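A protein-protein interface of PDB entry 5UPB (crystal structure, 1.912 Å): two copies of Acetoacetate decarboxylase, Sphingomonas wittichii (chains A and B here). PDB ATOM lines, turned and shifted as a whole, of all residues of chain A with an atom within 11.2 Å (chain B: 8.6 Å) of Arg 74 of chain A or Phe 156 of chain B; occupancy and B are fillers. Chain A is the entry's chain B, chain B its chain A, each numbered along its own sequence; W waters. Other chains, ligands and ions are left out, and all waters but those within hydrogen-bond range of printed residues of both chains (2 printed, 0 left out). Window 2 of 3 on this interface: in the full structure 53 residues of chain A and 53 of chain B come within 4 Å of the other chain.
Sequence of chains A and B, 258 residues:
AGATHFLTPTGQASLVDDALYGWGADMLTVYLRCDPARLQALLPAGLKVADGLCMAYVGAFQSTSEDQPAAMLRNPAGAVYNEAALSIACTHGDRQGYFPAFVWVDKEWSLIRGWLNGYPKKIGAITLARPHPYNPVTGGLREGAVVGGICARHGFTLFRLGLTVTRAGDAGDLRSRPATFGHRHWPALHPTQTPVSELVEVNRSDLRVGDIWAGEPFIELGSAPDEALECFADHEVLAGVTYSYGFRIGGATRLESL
The backbone carbonyl oxygen (O) of Glu 227 of chain B lies close to the side-chain amide oxygen (OE1) of Gln 12 of chain A (3.3 Å). The side-chain amide nitrogen (ND2) of Asn 75 of chain A is in hydrogen-bond range of the side-chain carboxylate (OD2) of Asp 226 of chain B, 2.9 Å away. The guanidinium group (NE) of Arg 153 of chain B is in salt-bridge range of the side-chain carboxylate (OE2) of Glu 108 of chain A, at 2.8 Å. NE1 of Trp 109 of chain A is in hydrogen-bond range of NE2 of His 154 of chain B.
NE1 of Trp 104 of chain B sits at hydrogen-bond distance from OE2 of Glu 227 of chain B. A ring nitrogen (ND1) of His 154 of chain B lies within hydrogen-bond range of the side-chain carboxylate (OD2) of Asp 226 of chain B. NH1 of Arg 153 of chain B sits at hydrogen-bond distance from ND1 of His 154 of chain B (3.5 Å). The guanidinium group (NH1) of Arg 153 of chain B lies within salt-bridge range of the side-chain carboxylate (OE2) of Glu 227 of chain B (3.6 Å).
O of Pro 225 of chain B touches OE1 of Gln 12 of chain A, at 3.8 Å. CZ of Phe 156 of chain B touches O of Arg 74 of chain A, at 3.4 Å. Arg 74 of chain A touches Pro 225 of chain B (O to CG, 3.8 Å). His 154 of chain B touches Asn 75 of chain A. CE2 of Phe 156 of chain B touches OD1 of Asn 75 of chain A (3.6 Å). Pro 225 of chain B touches Asn 75 of chain A (CG to CB, 3.8 Å). Ala 77 of chain A touches His 154 of chain B. Gly 78 of chain A touches His 154 of chain B (CA to CE1, 3.8 Å). CD1 of Trp 109 of chain A touches NH2 of Arg 153 of chain B, at 3.6 Å.
Printed residues of chain B within 4 Å of Gln 12 of chain A: Pro 225, Asp 226 and Glu 227. Met 72 of chain A touches none of the printed residues of chain B. Printed residues of chain B within 4 Å of Arg 74 of chain A: Phe 156 and Pro 225. No residue of chain A comes within 4 Å of Ala 152 of chain B. Of the printed residues of chain A, His 154 of chain B touches Asn 75, Ala 77, Gly 78 and Trp 109. No residue of chain A comes within 4 Å of Gly 155 of chain B. Of chain A, only Arg 74 and Asn 75 come within 4 Å of Phe 156 of chain B. Thr 157 of chain B touches none of the printed residues of chain A. Leu 158 of chain B touches none of the printed residues of chain A. No residue of chain A comes within 4 Å of Ser 223 of chain B. No residue of chain A comes within 4 Å of Ala 224 of chain B. Printed residues of chain A within 4 Å of Asp 226 of chain B: Gln 12 and Asn 75.
Along chain B the printed residues that touch a printed residue of chain A span positions 153 to 227. Hydrophobic or aromatic side chains of chain A within 4 Å of the printed part of chain B: Ala 77 and Trp 109. Among the printed residues, 14 pairs touch across the chains. Among the printed residues, Asp or Glu carboxylates within 4 Å of a Lys or Arg side-chain nitrogen of the other chain: Glu 108 of chain A with Arg 153 of chain B (2.8 Å).
No position is printed for both chains. Of the 14 pairs that touch across the chains among the printed residues, none has its exchanged pair printed and touching as well.
Water W1 lies within hydrogen-bond range of OE1 of Glu 108 of chain A (2.6 Å), NE2 of His 154 of chain B (2.7 Å) and NE1 of Trp 109 of chain A (3.5 Å). Water W2 lies within hydrogen-bond range of OD1 of Asn 75 of chain A (2.7 Å), N of Ala 77 of chain A (2.9 Å) and O of His 154 of chain B (2.9 Å).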
ATOM      1  N   GLN A  12     -23.989  27.262 -12.661  1.00  0.00           N
ATOM      2  CA  GLN A  12     -23.622  26.927 -14.031  1.00  0.00           C
ATOM      3  C   GLN A  12     -24.249  25.622 -14.519  1.00  0.00           C
ATOM      4  O   GLN A  12     -24.430  25.451 -15.731  1.00  0.00           O
ATOM      5  CB  GLN A  12     -22.099  26.857 -14.147  1.00  0.00           C
ATOM      6  CG  GLN A  12     -21.442  25.832 -13.202  1.00  0.00           C
ATOM      7  CD  GLN A  12     -20.059  25.417 -13.662  1.00  0.00           C
ATOM      8  OE1 GLN A  12     -19.647  25.720 -14.786  1.00  0.00           O
ATOM      9  NE2 GLN A  12     -19.336  24.718 -12.800  1.00  0.00           N
ATOM     10  N   SER A  63     -32.461  29.799 -29.258  1.00  0.00           N
ATOM     11  CA  SER A  63     -32.709  30.625 -28.082  1.00  0.00           C
ATOM     12  C   SER A  63     -31.397  31.107 -27.462  1.00  0.00           C
ATOM     13  O   SER A  63     -30.355  30.463 -27.558  1.00  0.00           O
ATOM     14  CB  SER A  63     -33.504  29.876 -27.018  1.00  0.00           C
ATOM     15  OG  SER A  63     -32.740  28.774 -26.532  1.00  0.00           O
ATOM     16  N   THR A  64     -31.469  32.295 -26.865  1.00  0.00           N
ATOM     17  CA  THR A  64     -30.330  32.985 -26.277  1.00  0.00           C
ATOM     18  C   THR A  64     -30.740  33.748 -25.035  1.00  0.00           C
ATOM     19  O   THR A  64     -31.742  34.471 -25.044  1.00  0.00           O
ATOM     20  CB  THR A  64     -29.675  33.949 -27.252  1.00  0.00           C
ATOM     21  OG1 THR A  64     -29.304  33.237 -28.427  1.00  0.00           O
ATOM     22  CG2 THR A  64     -28.418  34.619 -26.609  1.00  0.00           C
ATOM     23  N   GLN A  68     -26.385  35.659 -20.894  1.00  0.00           N
ATOM     24  CA  GLN A  68     -25.214  35.036 -21.515  1.00  0.00           C
ATOM     25  C   GLN A  68     -25.380  35.047 -23.019  1.00  0.00           C
ATOM     26  O   GLN A  68     -25.515  33.993 -23.658  1.00  0.00           O
ATOM     27  CB  GLN A  68     -25.000  33.601 -21.035  1.00  0.00           C
ATOM     28  CG  GLN A  68     -25.596  33.274 -19.713  1.00  0.00           C
ATOM     29  CD  GLN A  68     -24.910  32.092 -19.106  1.00  0.00           C
ATOM     30  OE1 GLN A  68     -25.333  30.951 -19.287  1.00  0.00           O
ATOM     31  NE2 GLN A  68     -23.819  32.352 -18.397  1.00  0.00           N
ATOM     32  N   PRO A  69     -25.336  36.228 -23.626  1.00  0.00           N
ATOM     33  CA  PRO A  69     -25.665  36.324 -25.049  1.00  0.00           C
ATOM     34  C   PRO A  69     -24.641  35.657 -25.946  1.00  0.00           C
ATOM     35  O   PRO A  69     -24.934  35.424 -27.123  1.00  0.00           O
ATOM     36  CB  PRO A  69     -25.729  37.850 -25.295  1.00  0.00           C
ATOM     37  CG  PRO A  69     -24.784  38.425 -24.277  1.00  0.00           C
ATOM     38  CD  PRO A  69     -24.909  37.519 -23.055  1.00  0.00           C
ATOM     39  N   ALA A  70     -23.445  35.353 -25.447  1.00  0.00           N
ATOM     40  CA  ALA A  70     -22.429  34.702 -26.264  1.00  0.00           C
ATOM     41  C   ALA A  70     -22.256  33.212 -25.916  1.00  0.00           C
ATOM     42  O   ALA A  70     -21.304  32.576 -26.376  1.00  0.00           O
ATOM     43  CB  ALA A  70     -21.095  35.438 -26.096  1.00  0.00           C
ATOM     44  N   ALA A  71     -23.204  32.622 -25.188  1.00  0.00           N
ATOM     45  CA  ALA A  71     -23.033  31.231 -24.734  1.00  0.00           C
ATOM     46  C   ALA A  71     -22.933  30.262 -25.898  1.00  0.00           C
ATOM     47  O   ALA A  71     -22.333  29.182 -25.783  1.00  0.00           O
ATOM     48  CB  ALA A  71     -24.221  30.818 -23.870  1.00  0.00           C
ATOM     49  N   MET A  72     -23.534  30.636 -27.013  1.00  0.00           N
ATOM     50  CA  MET A  72     -23.561  29.813 -28.213  1.00  0.00           C
ATOM     51  C   MET A  72     -22.164  29.492 -28.727  1.00  0.00           C
ATOM     52  O   MET A  72     -21.976  28.476 -29.411  1.00  0.00           O
ATOM     53  CB  MET A  72     -24.336  30.589 -29.283  1.00  0.00           C
ATOM     54  CG  MET A  72     -24.077  30.156 -30.696  1.00  0.00           C
ATOM     55  SD  MET A  72     -25.155  31.009 -31.873  1.00  0.00           S
ATOM     56  CE  MET A  72     -25.285  32.694 -31.185  1.00  0.00           C
ATOM     57  N   LEU A  73     -21.193  30.383 -28.453  1.00  0.00           N
ATOM     58  CA  LEU A  73     -19.827  30.213 -28.940  1.00  0.00           C
ATOM     59  C   LEU A  73     -19.208  28.926 -28.381  1.00  0.00           C
ATOM     60  O   LEU A  73     -18.474  28.225 -29.085  1.00  0.00           O
ATOM     61  CB  LEU A  73     -18.975  31.412 -28.543  1.00  0.00           C
ATOM     62  CG  LEU A  73     -17.490  31.425 -28.909  1.00  0.00           C
ATOM     63  CD1 LEU A  73     -17.349  31.544 -30.401  1.00  0.00           C
ATOM     64  CD2 LEU A  73     -16.741  32.581 -28.248  1.00  0.00           C
ATOM     65  N   ARG A  74     -19.420  28.657 -27.094  1.00  0.00           N
ATOM     66  CA  ARG A  74     -18.812  27.502 -26.424  1.00  0.00           C
ATOM     67  C   ARG A  74     -19.788  26.331 -26.223  1.00  0.00           C
ATOM     68  O   ARG A  74     -19.346  25.220 -25.899  1.00  0.00           O
ATOM     69  CB  ARG A  74     -18.199  27.954 -25.108  1.00  0.00           C
ATOM     70  CG  ARG A  74     -16.939  28.789 -25.431  1.00  0.00           C
ATOM     71  CD  ARG A  74     -16.178  29.468 -24.287  1.00  0.00           C
ATOM     72  NE  ARG A  74     -15.093  30.277 -24.865  1.00  0.00           N
ATOM     73  CZ  ARG A  74     -13.912  29.811 -25.282  1.00  0.00           C
ATOM     74  NH1 ARG A  74     -13.610  28.519 -25.195  1.00  0.00           N
ATOM     75  NH2 ARG A  74     -13.029  30.650 -25.813  1.00  0.00           N
ATOM     76  N   ASN A  75     -21.092  26.564 -26.375  1.00  0.00           N
ATOM     77  CA  ASN A  75     -22.123  25.557 -26.127  1.00  0.00           C
ATOM     78  C   ASN A  75     -23.200  25.654 -27.185  1.00  0.00           C
ATOM     79  O   ASN A  75     -24.347  26.034 -26.904  1.00  0.00           O
ATOM     80  CB  ASN A  75     -22.720  25.714 -24.731  1.00  0.00           C
ATOM     81  CG  ASN A  75     -23.533  24.494 -24.321  1.00  0.00           C
ATOM     82  OD1 ASN A  75     -23.603  23.516 -25.073  1.00  0.00           O
ATOM     83  ND2 ASN A  75     -24.082  24.518 -23.111  1.00  0.00           N
ATOM     84  N   PRO A  76     -22.868  25.285 -28.422  1.00  0.00           N
ATOM     85  CA  PRO A  76     -23.852  25.391 -29.515  1.00  0.00           C
ATOM     86  C   PRO A  76     -25.078  24.521 -29.351  1.00  0.00           C
ATOM     87  O   PRO A  76     -26.177  24.946 -29.738  1.00  0.00           O
ATOM     88  CB  PRO A  76     -23.030  25.009 -30.761  1.00  0.00           C
ATOM     89  CG  PRO A  76     -21.811  24.328 -30.256  1.00  0.00           C
ATOM     90  CD  PRO A  76     -21.530  24.919 -28.908  1.00  0.00           C
ATOM     91  N   ALA A  77     -24.924  23.294 -28.837  1.00  0.00           N
ATOM     92  CA  ALA A  77     -26.084  22.432 -28.669  1.00  0.00           C
ATOM     93  C   ALA A  77     -27.027  22.960 -27.590  1.00  0.00           C
ATOM     94  O   ALA A  77     -28.200  22.569 -27.563  1.00  0.00           O
ATOM     95  CB  ALA A  77     -25.628  20.999 -28.369  1.00  0.00           C
ATOM     96  N   GLY A  78     -26.542  23.845 -26.705  1.00  0.00           N
ATOM     97  CA  GLY A  78     -27.417  24.499 -25.761  1.00  0.00           C
ATOM     98  C   GLY A  78     -28.165  25.690 -26.327  1.00  0.00           C
ATOM     99  O   GLY A  78     -28.881  26.369 -25.589  1.00  0.00           O
ATOM    100  N   ALA A  79     -28.026  25.964 -27.614  1.00  0.00           N
ATOM    101  CA  ALA A  79     -28.604  27.184 -28.202  1.00  0.00           C
ATOM    102  C   ALA A  79     -29.623  26.928 -29.307  1.00  0.00           C
ATOM    103  O   ALA A  79     -30.223  27.892 -29.838  1.00  0.00           O
ATOM    104  CB  ALA A  79     -27.486  28.090 -28.721  1.00  0.00           C
ATOM    105  N   VAL A  80     -29.842  25.672 -29.672  1.00  0.00           N
ATOM    106  CA  VAL A  80     -30.752  25.335 -30.746  1.00  0.00           C
ATOM    107  C   VAL A  80     -31.586  24.142 -30.328  1.00  0.00           C
ATOM    108  O   VAL A  80     -31.112  23.257 -29.614  1.00  0.00           O
ATOM    109  CB  VAL A  80     -29.976  25.035 -32.054  1.00  0.00           C
ATOM    110  CG1 VAL A  80     -29.325  26.318 -32.561  1.00  0.00           C
ATOM    111  CG2 VAL A  80     -28.939  23.954 -31.844  1.00  0.00           C
ATOM    112  N   LYS A 107     -34.603  18.930 -26.959  1.00  0.00           N
ATOM    113  CA  LYS A 107     -33.641  19.357 -25.944  1.00  0.00           C
ATOM    114  C   LYS A 107     -34.388  19.476 -24.621  1.00  0.00           C
ATOM    115  O   LYS A 107     -35.366  20.229 -24.528  1.00  0.00           O
ATOM    116  CB  LYS A 107     -32.994  20.696 -26.334  1.00  0.00           C
ATOM    117  CG  LYS A 107     -32.103  20.640 -27.552  1.00  0.00           C
ATOM    118  CD  LYS A 107     -30.793  19.824 -27.277  1.00  0.00           C
ATOM    119  CE  LYS A 107     -30.024  19.532 -28.544  1.00  0.00           C
ATOM    120  NZ  LYS A 107     -29.698  20.847 -29.259  1.00  0.00           N
ATOM    121  N   GLU A 108     -33.871  18.826 -23.562  1.00  0.00           N
ATOM    122  CA  GLU A 108     -34.634  18.776 -22.316  1.00  0.00           C
ATOM    123  C   GLU A 108     -34.639  20.108 -21.590  1.00  0.00           C
ATOM    124  O   GLU A 108     -35.539  20.339 -20.771  1.00  0.00           O
ATOM    125  CB  GLU A 108     -34.117  17.650 -21.372  1.00  0.00           C
ATOM    126  CG  GLU A 108     -33.042  18.022 -20.373  1.00  0.00           C
ATOM    127  CD  GLU A 108     -31.691  18.264 -21.001  1.00  0.00           C
ATOM    128  OE1 GLU A 108     -31.563  19.199 -21.821  1.00  0.00           O
ATOM    129  OE2 GLU A 108     -30.736  17.529 -20.660  1.00  0.00           O
ATOM    130  N   TRP A 109     -33.675  20.993 -21.851  1.00  0.00           N
ATOM    131  CA  TRP A 109     -33.789  22.326 -21.259  1.00  0.00           C
ATOM    132  C   TRP A 109     -35.002  23.059 -21.790  1.00  0.00           C
ATOM    133  O   TRP A 109     -35.629  23.832 -21.044  1.00  0.00           O
ATOM    134  CB  TRP A 109     -32.518  23.158 -21.475  1.00  0.00           C
ATOM    135  CG  TRP A 109     -31.845  23.046 -22.842  1.00  0.00           C
ATOM    136  CD1 TRP A 109     -30.850  22.163 -23.194  1.00  0.00           C
ATOM    137  CD2 TRP A 109     -32.057  23.881 -23.992  1.00  0.00           C
ATOM    138  NE1 TRP A 109     -30.464  22.371 -24.500  1.00  0.00           N
ATOM    139  CE2 TRP A 109     -31.185  23.416 -25.011  1.00  0.00           C
ATOM    140  CE3 TRP A 109     -32.898  24.972 -24.263  1.00  0.00           C
ATOM    141  CZ2 TRP A 109     -31.132  23.990 -26.274  1.00  0.00           C
ATOM    142  CZ3 TRP A 109     -32.850  25.542 -25.541  1.00  0.00           C
ATOM    143  CH2 TRP A 109     -31.978  25.047 -26.531  1.00  0.00           C
ATOM    144  N   TRP B 104     -27.684  11.596 -15.507  1.00  0.00           N
ATOM    145  CA  TRP B 104     -28.039  11.727 -16.918  1.00  0.00           C
ATOM    146  C   TRP B 104     -28.705  10.424 -17.352  1.00  0.00           C
ATOM    147  O   TRP B 104     -28.206   9.338 -17.038  1.00  0.00           O
ATOM    148  CB  TRP B 104     -26.805  12.030 -17.804  1.00  0.00           C
ATOM    149  CG  TRP B 104     -26.059  13.310 -17.433  1.00  0.00           C
ATOM    150  CD1 TRP B 104     -26.213  14.561 -18.013  1.00  0.00           C
ATOM    151  CD2 TRP B 104     -25.057  13.467 -16.413  1.00  0.00           C
ATOM    152  NE1 TRP B 104     -25.358  15.459 -17.419  1.00  0.00           N
ATOM    153  CE2 TRP B 104     -24.646  14.817 -16.432  1.00  0.00           C
ATOM    154  CE3 TRP B 104     -24.467  12.597 -15.490  1.00  0.00           C
ATOM    155  CZ2 TRP B 104     -23.680  15.318 -15.569  1.00  0.00           C
ATOM    156  CZ3 TRP B 104     -23.492  13.098 -14.631  1.00  0.00           C
ATOM    157  CH2 TRP B 104     -23.111  14.462 -14.688  1.00  0.00           C
ATOM    158  N   GLY B 124     -28.929  12.677 -21.444  1.00  0.00           N
ATOM    159  CA  GLY B 124     -27.654  12.497 -22.106  1.00  0.00           C
ATOM    160  C   GLY B 124     -27.688  11.269 -22.988  1.00  0.00           C
ATOM    161  O   GLY B 124     -28.704  10.598 -23.106  1.00  0.00           O
ATOM    162  N   ALA B 125     -26.554  10.985 -23.599  1.00  0.00           N
ATOM    163  CA  ALA B 125     -26.359   9.738 -24.323  1.00  0.00           C
ATOM    164  C   ALA B 125     -25.465   8.883 -23.443  1.00  0.00           C
ATOM    165  O   ALA B 125     -24.436   9.365 -22.966  1.00  0.00           O
ATOM    166  CB  ALA B 125     -25.711   9.995 -25.695  1.00  0.00           C
ATOM    167  N   ILE B 150     -19.892   5.025 -20.662  1.00  0.00           N
ATOM    168  CA  ILE B 150     -19.582   6.403 -21.026  1.00  0.00           C
ATOM    169  C   ILE B 150     -20.892   7.179 -21.102  1.00  0.00           C
ATOM    170  O   ILE B 150     -21.958   6.634 -21.414  1.00  0.00           O
ATOM    171  CB  ILE B 150     -18.798   6.472 -22.370  1.00  0.00           C
ATOM    172  CG1 ILE B 150     -18.278   7.878 -22.662  1.00  0.00           C
ATOM    173  CG2 ILE B 150     -19.693   6.084 -23.534  1.00  0.00           C
ATOM    174  CD1 ILE B 150     -17.169   7.866 -23.716  1.00  0.00           C
ATOM    175  N   CYS B 151     -20.823   8.452 -20.766  1.00  0.00           N
ATOM    176  CA  CYS B 151     -21.988   9.296 -20.945  1.00  0.00           C
ATOM    177  C   CYS B 151     -21.534  10.656 -21.446  1.00  0.00           C
ATOM    178  O   CYS B 151     -20.413  11.093 -21.180  1.00  0.00           O
ATOM    179  CB  CYS B 151     -22.793   9.430 -19.638  1.00  0.00           C
ATOM    180  SG  CYS B 151     -21.840   9.995 -18.255  1.00  0.00           S
ATOM    181  N   ALA B 152     -22.403  11.289 -22.220  1.00  0.00           N
ATOM    182  CA  ALA B 152     -22.094  12.556 -22.864  1.00  0.00           C
ATOM    183  C   ALA B 152     -23.374  13.371 -23.018  1.00  0.00           C
ATOM    184  O   ALA B 152     -24.480  12.821 -23.062  1.00  0.00           O
ATOM    185  CB  ALA B 152     -21.469  12.341 -24.238  1.00  0.00           C
ATOM    186  N   ARG B 153     -23.204  14.694 -23.125  1.00  0.00           N
ATOM    187  CA  ARG B 153     -24.338  15.584 -23.326  1.00  0.00           C
ATOM    188  C   ARG B 153     -23.873  16.811 -24.087  1.00  0.00           C
ATOM    189  O   ARG B 153     -22.793  17.339 -23.810  1.00  0.00           O
ATOM    190  CB  ARG B 153     -24.964  15.982 -21.984  1.00  0.00           C
ATOM    191  CG  ARG B 153     -26.144  16.957 -22.120  1.00  0.00           C
ATOM    192  CD  ARG B 153     -26.869  17.154 -20.768  1.00  0.00           C
ATOM    193  NE  ARG B 153     -27.970  18.111 -20.850  1.00  0.00           N
ATOM    194  CZ  ARG B 153     -27.838  19.430 -20.687  1.00  0.00           C
ATOM    195  NH1 ARG B 153     -26.650  19.978 -20.405  1.00  0.00           N
ATOM    196  NH2 ARG B 153     -28.906  20.221 -20.800  1.00  0.00           N
ATOM    197  N   HIS B 154     -24.687  17.258 -25.059  1.00  0.00           N
ATOM    198  CA  HIS B 154     -24.412  18.487 -25.830  1.00  0.00           C
ATOM    199  C   HIS B 154     -23.080  18.398 -26.563  1.00  0.00           C
ATOM    200  O   HIS B 154     -22.463  19.414 -26.894  1.00  0.00           O
ATOM    201  CB  HIS B 154     -24.439  19.721 -24.932  1.00  0.00           C
ATOM    202  CG  HIS B 154     -25.820  20.197 -24.599  1.00  0.00           C
ATOM    203  ND1 HIS B 154     -26.062  21.163 -23.638  1.00  0.00           N
ATOM    204  CD2 HIS B 154     -27.029  19.840 -25.090  1.00  0.00           C
ATOM    205  CE1 HIS B 154     -27.360  21.390 -23.569  1.00  0.00           C
ATOM    206  NE2 HIS B 154     -27.970  20.593 -24.429  1.00  0.00           N
ATOM    207  N   GLY B 155     -22.637  17.170 -26.834  1.00  0.00           N
ATOM    208  CA  GLY B 155     -21.378  16.915 -27.462  1.00  0.00           C
ATOM    209  C   GLY B 155     -20.196  16.792 -26.516  1.00  0.00           C
ATOM    210  O   GLY B 155     -19.091  16.521 -26.991  1.00  0.00           O
ATOM    211  N   PHE B 156     -20.384  16.987 -25.202  1.00  0.00           N
ATOM    212  CA  PHE B 156     -19.294  16.923 -24.245  1.00  0.00           C
ATOM    213  C   PHE B 156     -19.287  15.564 -23.552  1.00  0.00           C
ATOM    214  O   PHE B 156     -20.300  15.145 -22.990  1.00  0.00           O
ATOM    215  CB  PHE B 156     -19.415  18.007 -23.186  1.00  0.00           C
ATOM    216  CG  PHE B 156     -19.475  19.418 -23.754  1.00  0.00           C
ATOM    217  CD1 PHE B 156     -18.331  20.075 -24.125  1.00  0.00           C
ATOM    218  CD2 PHE B 156     -20.702  20.042 -23.936  1.00  0.00           C
ATOM    219  CE1 PHE B 156     -18.397  21.354 -24.657  1.00  0.00           C
ATOM    220  CE2 PHE B 156     -20.773  21.322 -24.460  1.00  0.00           C
ATOM    221  CZ  PHE B 156     -19.637  21.973 -24.836  1.00  0.00           C
ATOM    222  N   THR B 157     -18.138  14.909 -23.548  1.00  0.00           N
ATOM    223  CA  THR B 157     -17.978  13.759 -22.666  1.00  0.00           C
ATOM    224  C   THR B 157     -18.161  14.213 -21.223  1.00  0.00           C
ATOM    225  O   THR B 157     -17.508  15.151 -20.760  1.00  0.00           O
ATOM    226  CB  THR B 157     -16.591  13.157 -22.824  1.00  0.00           C
ATOM    227  OG1 THR B 157     -16.324  12.900 -24.219  1.00  0.00           O
ATOM    228  CG2 THR B 157     -16.543  11.857 -22.026  1.00  0.00           C
ATOM    229  N   LEU B 158     -19.045  13.537 -20.503  1.00  0.00           N
ATOM    230  CA  LEU B 158     -19.265  13.854 -19.096  1.00  0.00           C
ATOM    231  C   LEU B 158     -18.347  13.026 -18.202  1.00  0.00           C
ATOM    232  O   LEU B 158     -17.569  13.578 -17.414  1.00  0.00           O
ATOM    233  CB  LEU B 158     -20.723  13.591 -18.738  1.00  0.00           C
ATOM    234  CG  LEU B 158     -21.737  14.426 -19.547  1.00  0.00           C
ATOM    235  CD1 LEU B 158     -23.113  13.765 -19.424  1.00  0.00           C
ATOM    236  CD2 LEU B 158     -21.726  15.857 -19.072  1.00  0.00           C
ATOM    237  N   PHE B 159     -18.440  11.700 -18.290  1.00  0.00           N
ATOM    238  CA  PHE B 159     -17.407  10.878 -17.671  1.00  0.00           C
ATOM    239  C   PHE B 159     -17.365   9.511 -18.327  1.00  0.00           C
ATOM    240  O   PHE B 159     -18.249   9.139 -19.102  1.00  0.00           O
ATOM    241  CB  PHE B 159     -17.585  10.768 -16.148  1.00  0.00           C
ATOM    242  CG  PHE B 159     -18.814  10.030 -15.680  1.00  0.00           C
ATOM    243  CD1 PHE B 159     -18.781   8.652 -15.430  1.00  0.00           C
ATOM    244  CD2 PHE B 159     -19.994  10.719 -15.418  1.00  0.00           C
ATOM    245  CE1 PHE B 159     -19.904   7.980 -14.951  1.00  0.00           C
ATOM    246  CE2 PHE B 159     -21.125  10.049 -14.946  1.00  0.00           C
ATOM    247  CZ  PHE B 159     -21.064   8.660 -14.698  1.00  0.00           C
ATOM    248  N   GLY B 222     -14.942  14.320 -17.497  1.00  0.00           N
ATOM    249  CA  GLY B 222     -14.830  15.347 -18.510  1.00  0.00           C
ATOM    250  C   GLY B 222     -15.121  16.732 -17.968  1.00  0.00           C
ATOM    251  O   GLY B 222     -15.086  16.985 -16.758  1.00  0.00           O
ATOM    252  N   SER B 223     -15.477  17.639 -18.878  1.00  0.00           N
ATOM    253  CA  SER B 223     -15.821  18.988 -18.467  1.00  0.00           C
ATOM    254  C   SER B 223     -16.786  19.560 -19.496  1.00  0.00           C
ATOM    255  O   SER B 223     -16.685  19.238 -20.676  1.00  0.00           O
ATOM    256  CB  SER B 223     -14.542  19.847 -18.394  1.00  0.00           C
ATOM    257  OG  SER B 223     -14.819  21.207 -18.166  1.00  0.00           O
ATOM    258  N   ALA B 224     -17.740  20.366 -19.036  1.00  0.00           N
ATOM    259  CA  ALA B 224     -18.687  21.016 -19.934  1.00  0.00           C
ATOM    260  C   ALA B 224     -19.058  22.397 -19.409  1.00  0.00           C
ATOM    261  O   ALA B 224     -19.118  22.604 -18.192  1.00  0.00           O
ATOM    262  CB  ALA B 224     -19.945  20.153 -20.102  1.00  0.00           C
ATOM    263  N   PRO B 225     -19.344  23.348 -20.293  1.00  0.00           N
ATOM    264  CA  PRO B 225     -19.692  24.702 -19.822  1.00  0.00           C
ATOM    265  C   PRO B 225     -20.987  24.751 -19.019  1.00  0.00           C
ATOM    266  O   PRO B 225     -21.154  25.693 -18.238  1.00  0.00           O
ATOM    267  CB  PRO B 225     -19.796  25.513 -21.117  1.00  0.00           C
ATOM    268  CG  PRO B 225     -20.094  24.499 -22.200  1.00  0.00           C
ATOM    269  CD  PRO B 225     -19.381  23.217 -21.756  1.00  0.00           C
ATOM    270  N   ASP B 226     -21.899  23.773 -19.172  1.00  0.00           N
ATOM    271  CA  ASP B 226     -23.181  23.752 -18.460  1.00  0.00           C
ATOM    272  C   ASP B 226     -23.282  22.598 -17.451  1.00  0.00           C
ATOM    273  O   ASP B 226     -24.378  22.154 -17.088  1.00  0.00           O
ATOM    274  CB  ASP B 226     -24.347  23.720 -19.460  1.00  0.00           C
ATOM    275  CG  ASP B 226     -24.257  22.585 -20.479  1.00  0.00           C
ATOM    276  OD1 ASP B 226     -23.275  21.807 -20.449  1.00  0.00           O
ATOM    277  OD2 ASP B 226     -25.163  22.500 -21.339  1.00  0.00           O
ATOM    278  N   GLU B 227     -22.143  22.117 -16.965  1.00  0.00           N
ATOM    279  CA  GLU B 227     -22.098  21.088 -15.933  1.00  0.00           C
ATOM    280  C   GLU B 227     -21.100  21.535 -14.886  1.00  0.00           C
ATOM    281  O   GLU B 227     -20.335  22.471 -15.105  1.00  0.00           O
ATOM    282  CB  GLU B 227     -21.665  19.732 -16.491  1.00  0.00           C
ATOM    283  CG  GLU B 227     -22.507  19.218 -17.633  1.00  0.00           C
ATOM    284  CD  GLU B 227     -23.867  18.732 -17.176  1.00  0.00           C
ATOM    285  OE1 GLU B 227     -24.198  18.898 -15.970  1.00  0.00           O
ATOM    286  OE2 GLU B 227     -24.613  18.163 -18.015  1.00  0.00           O
ATOM    287  N   LEU B 229     -18.810  19.178 -13.280  1.00  0.00           N
ATOM    288  CA  LEU B 229     -18.124  17.912 -13.055  1.00  0.00           C
ATOM    289  C   LEU B 229     -16.864  18.099 -12.234  1.00  0.00           C
ATOM    290  O   LEU B 229     -16.438  17.166 -11.559  1.00  0.00           O
ATOM    291  CB  LEU B 229     -17.790  17.267 -14.398  1.00  0.00           C
ATOM    292  CG  LEU B 229     -19.024  16.869 -15.194  1.00  0.00           C
ATOM    293  CD1 LEU B 229     -18.744  16.811 -16.702  1.00  0.00           C
ATOM    294  CD2 LEU B 229     -19.509  15.527 -14.688  1.00  0.00           C
HETATM  295  O   HOH W   1     -30.139  18.961 -24.007  1.00  0.00           O
HETATM  296  O   HOH W   2     -22.674  22.314 -27.297  1.00  0.00           O
